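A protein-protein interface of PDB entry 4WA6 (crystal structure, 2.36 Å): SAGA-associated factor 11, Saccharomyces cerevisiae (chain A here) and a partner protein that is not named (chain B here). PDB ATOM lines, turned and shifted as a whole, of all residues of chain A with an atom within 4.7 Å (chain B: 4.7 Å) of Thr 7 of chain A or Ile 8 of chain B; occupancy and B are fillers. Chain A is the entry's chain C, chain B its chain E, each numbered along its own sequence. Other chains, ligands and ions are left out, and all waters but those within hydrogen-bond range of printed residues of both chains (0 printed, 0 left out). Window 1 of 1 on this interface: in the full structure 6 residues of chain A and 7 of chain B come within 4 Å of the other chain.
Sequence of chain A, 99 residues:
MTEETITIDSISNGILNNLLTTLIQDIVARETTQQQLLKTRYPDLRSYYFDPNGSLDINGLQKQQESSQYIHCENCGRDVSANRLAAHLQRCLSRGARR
Glu 7 of chain B touches Ile 6 of chain A. Gly 4 of chain B touches Thr 7 of chain A. Thr 7 of chain A touches Asp 5 of chain B. Thr 7 of chain A touches Ala 6 of chain B (CA to O, 3.3 Å). Glu 7 of chain B touches Thr 7 of chain A. CD1 of Ile 8 of chain B touches C of Thr 7 of chain A (3.7 Å). O of Ala 6 of chain B touches N of Ile 8 of chain A, 3.7 Å away. Ile 8 of chain A touches Ile 8 of chain B.
N of Asp 5 of chain B sits at hydrogen-bond distance from OD2 of Asp 9 of chain A, at 3.5 Å. The backbone carbonyl oxygen (O) of Gly 4 of chain B is in hydrogen-bond range of the backbone NH (N) of Asp 9 of chain A (2.9 Å). N of Ile 8 of chain B is in hydrogen-bond range of O of Ile 6 of chain A (2.8 Å). OG1 of Thr 5 of chain A sits at hydrogen-bond distance from OE2 of Glu 7 of chain B. The backbone NH (N) of Ile 8 of chain A is in hydrogen-bond range of the backbone carbonyl oxygen (O) of Gly 4 of chain B, 3.3 Å away.
Thr 7 of chain A touches just these residues of chain B: Gly 4, Asp 5, Ala 6, Glu 7 and Ile 8. Of chain A, only Ile 6, Thr 7 and Ile 8 come within 4 Å of Ile 8 of chain B. Of the printed residues of chain A, Gly 4 of chain B touches Thr 7, Ile 8 and Asp 9. Printed residues of chain B within 4 Å of Ile 6 of chain A: Glu 7 (3.3 Å) and Ile 8 (2.8 Å). Printed residues of chain B within 4 Å of Ile 8 of chain A: Gly 4, Ala 6 and Ile 8. Gly 10 of chain B touches none of the printed residues of chain A.
Of the 7 printed residues of chain A, 5 touch a printed residue of chain B.
OG1 of Thr 7 of chain A lies close to N of Asp 9 of chain A (3.3 Å). The side-chain hydroxyl (OG1) of Thr 7 of chain A is in hydrogen-bond range of the backbone NH (N) of Ser 10 of chain A, 3.0 Å away.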
ATOM      1  N   THR A   5      20.685  -7.686  -5.179  1.00  0.00           N
ATOM      2  CA  THR A   5      20.006  -6.755  -6.141  1.00  0.00           C
ATOM      3  C   THR A   5      19.090  -5.751  -5.396  1.00  0.00           C
ATOM      4  O   THR A   5      19.512  -5.231  -4.365  1.00  0.00           O
ATOM      5  CB  THR A   5      19.262  -7.533  -7.242  1.00  0.00           C
ATOM      6  OG1 THR A   5      18.367  -8.480  -6.623  1.00  0.00           O
ATOM      7  CG2 THR A   5      20.299  -8.224  -8.196  1.00  0.00           C
ATOM      8  N   ILE A   6      17.882  -5.442  -5.889  1.00  0.00           N
ATOM      9  CA  ILE A   6      17.159  -4.316  -5.305  1.00  0.00           C
ATOM     10  C   ILE A   6      15.832  -4.687  -4.694  1.00  0.00           C
ATOM     11  O   ILE A   6      15.132  -5.529  -5.204  1.00  0.00           O
ATOM     12  CB  ILE A   6      17.005  -3.124  -6.275  1.00  0.00           C
ATOM     13  CG1 ILE A   6      16.185  -3.476  -7.520  1.00  0.00           C
ATOM     14  CG2 ILE A   6      18.380  -2.580  -6.668  1.00  0.00           C
ATOM     15  CD1 ILE A   6      15.671  -2.236  -8.241  1.00  0.00           C
ATOM     16  N   THR A   7      15.535  -4.072  -3.562  1.00  0.00           N
ATOM     17  CA  THR A   7      14.315  -4.295  -2.841  1.00  0.00           C
ATOM     18  C   THR A   7      13.784  -2.955  -2.384  1.00  0.00           C
ATOM     19  O   THR A   7      14.436  -1.922  -2.535  1.00  0.00           O
ATOM     20  CB  THR A   7      14.588  -5.102  -1.598  1.00  0.00           C
ATOM     21  OG1 THR A   7      15.436  -4.320  -0.748  1.00  0.00           O
ATOM     22  CG2 THR A   7      15.261  -6.420  -1.961  1.00  0.00           C
ATOM     23  N   ILE A   8      12.596  -2.961  -1.826  1.00  0.00           N
ATOM     24  CA  ILE A   8      11.997  -1.726  -1.350  1.00  0.00           C
ATOM     25  C   ILE A   8      12.885  -1.140  -0.261  1.00  0.00           C
ATOM     26  O   ILE A   8      13.088   0.063  -0.208  1.00  0.00           O
ATOM     27  CB  ILE A   8      10.570  -1.950  -0.809  1.00  0.00           C
ATOM     28  CG1 ILE A   8       9.651  -2.557  -1.884  1.00  0.00           C
ATOM     29  CG2 ILE A   8       9.949  -0.663  -0.287  1.00  0.00           C
ATOM     30  CD1 ILE A   8       9.148  -1.541  -2.879  1.00  0.00           C
ATOM     31  N   ASP A   9      13.439  -1.998   0.593  1.00  0.00           N
ATOM     32  CA  ASP A   9      14.252  -1.512   1.699  1.00  0.00           C
ATOM     33  C   ASP A   9      15.538  -0.947   1.219  1.00  0.00           C
ATOM     34  O   ASP A   9      15.910   0.114   1.628  1.00  0.00           O
ATOM     35  CB  ASP A   9      14.555  -2.599   2.680  1.00  0.00           C
ATOM     36  CG  ASP A   9      13.351  -3.016   3.422  1.00  0.00           C
ATOM     37  OD1 ASP A   9      12.417  -2.183   3.546  1.00  0.00           O
ATOM     38  OD2 ASP A   9      13.312  -4.199   3.856  1.00  0.00           O
ATOM     39  N   SER A  10      16.206  -1.654   0.330  1.00  0.00           N
ATOM     40  CA  SER A  10      17.490  -1.208  -0.102  1.00  0.00           C
ATOM     41  C   SER A  10      17.348   0.120  -0.830  1.00  0.00           C
ATOM     42  O   SER A  10      18.098   1.030  -0.530  1.00  0.00           O
ATOM     43  CB  SER A  10      18.180  -2.256  -0.959  1.00  0.00           C
ATOM     44  OG  SER A  10      17.708  -2.198  -2.289  1.00  0.00           O
ATOM     45  N   ILE A  11      16.367   0.249  -1.730  1.00  0.00           N
ATOM     46  CA  ILE A  11      16.150   1.494  -2.486  1.00  0.00           C
ATOM     47  C   ILE A  11      15.728   2.661  -1.608  1.00  0.00           C
ATOM     48  O   ILE A  11      16.230   3.762  -1.754  1.00  0.00           O
ATOM     49  CB  ILE A  11      15.094   1.329  -3.604  1.00  0.00           C
ATOM     50  CG1 ILE A  11      15.552   0.346  -4.654  1.00  0.00           C
ATOM     51  CG2 ILE A  11      14.760   2.644  -4.284  1.00  0.00           C
ATOM     52  CD1 ILE A  11      16.655   0.841  -5.526  1.00  0.00           C
ATOM     53  N   GLY B   4       8.984  -4.927   2.519  1.00  0.00           N
ATOM     54  CA  GLY B   4      10.261  -4.268   2.362  1.00  0.00           C
ATOM     55  C   GLY B   4      11.355  -5.142   1.773  1.00  0.00           C
ATOM     56  O   GLY B   4      12.231  -4.649   1.037  1.00  0.00           O
ATOM     57  N   ASP B   5      11.320  -6.437   2.090  1.00  0.00           N
ATOM     58  CA  ASP B   5      12.343  -7.373   1.596  1.00  0.00           C
ATOM     59  C   ASP B   5      12.062  -7.919   0.187  1.00  0.00           C
ATOM     60  O   ASP B   5      12.856  -8.652  -0.368  1.00  0.00           O
ATOM     61  CB  ASP B   5      12.553  -8.523   2.581  1.00  0.00           C
ATOM     62  CG  ASP B   5      12.791  -8.042   4.011  1.00  0.00           C
ATOM     63  OD1 ASP B   5      13.375  -6.948   4.195  1.00  0.00           O
ATOM     64  OD2 ASP B   5      12.391  -8.755   4.960  1.00  0.00           O
ATOM     65  N   ALA B   6      10.955  -7.549  -0.424  1.00  0.00           N
ATOM     66  CA  ALA B   6      10.666  -8.119  -1.726  1.00  0.00           C
ATOM     67  C   ALA B   6      11.604  -7.574  -2.814  1.00  0.00           C
ATOM     68  O   ALA B   6      11.790  -6.390  -2.941  1.00  0.00           O
ATOM     69  CB  ALA B   6       9.205  -7.901  -2.093  1.00  0.00           C
ATOM     70  N   GLU B   7      12.179  -8.468  -3.603  1.00  0.00           N
ATOM     71  CA  GLU B   7      12.988  -8.055  -4.726  1.00  0.00           C
ATOM     72  C   GLU B   7      12.128  -7.305  -5.734  1.00  0.00           C
ATOM     73  O   GLU B   7      11.046  -7.743  -6.095  1.00  0.00           O
ATOM     74  CB  GLU B   7      13.621  -9.266  -5.383  1.00  0.00           C
ATOM     75  CG  GLU B   7      14.487  -8.926  -6.578  1.00  0.00           C
ATOM     76  CD  GLU B   7      15.108 -10.165  -7.202  1.00  0.00           C
ATOM     77  OE1 GLU B   7      14.361 -11.114  -7.551  1.00  0.00           O
ATOM     78  OE2 GLU B   7      16.346 -10.178  -7.350  1.00  0.00           O
ATOM     79  N   ILE B   8      12.627  -6.177  -6.191  1.00  0.00           N
ATOM     80  CA  ILE B   8      11.923  -5.374  -7.159  1.00  0.00           C
ATOM     81  C   ILE B   8      12.054  -5.931  -8.599  1.00  0.00           C
ATOM     82  O   ILE B   8      13.128  -5.942  -9.191  1.00  0.00           O
ATOM     83  CB  ILE B   8      12.417  -3.929  -7.083  1.00  0.00           C
ATOM     84  CG1 ILE B   8      12.000  -3.338  -5.740  1.00  0.00           C
ATOM     85  CG2 ILE B   8      11.864  -3.117  -8.240  1.00  0.00           C
ATOM     86  CD1 ILE B   8      12.298  -1.864  -5.559  1.00  0.00           C
ATOM     87  N   LYS B   9      10.935  -6.385  -9.143  1.00  0.00           N
ATOM     88  CA  LYS B   9      10.847  -6.828 -10.538  1.00  0.00           C
ATOM     89  C   LYS B   9      11.153  -5.744 -11.594  1.00  0.00           C
ATOM     90  O   LYS B   9      11.939  -5.943 -12.508  1.00  0.00           O
ATOM     91  CB  LYS B   9       9.429  -7.365 -10.791  1.00  0.00           C
ATOM     92  CG  LYS B   9       9.382  -8.677 -11.546  1.00  0.00           C
ATOM     93  CD  LYS B   9       7.942  -9.161 -11.674  1.00  0.00           C
ATOM     94  CE  LYS B   9       7.821 -10.651 -11.402  1.00  0.00           C
ATOM     95  NZ  LYS B   9       6.414 -11.006 -11.090  1.00  0.00           N
ATOM     96  N   GLY B  10      10.500  -4.594 -11.460  1.00  0.00           N
ATOM     97  CA  GLY B  10      10.481  -3.554 -12.499  1.00  0.00           C
ATOM     98  C   GLY B  10       9.484  -2.482 -12.116  1.00  0.00           C
ATOM     99  O   GLY B  10       8.864  -2.553 -11.083  1.00  0.00           O
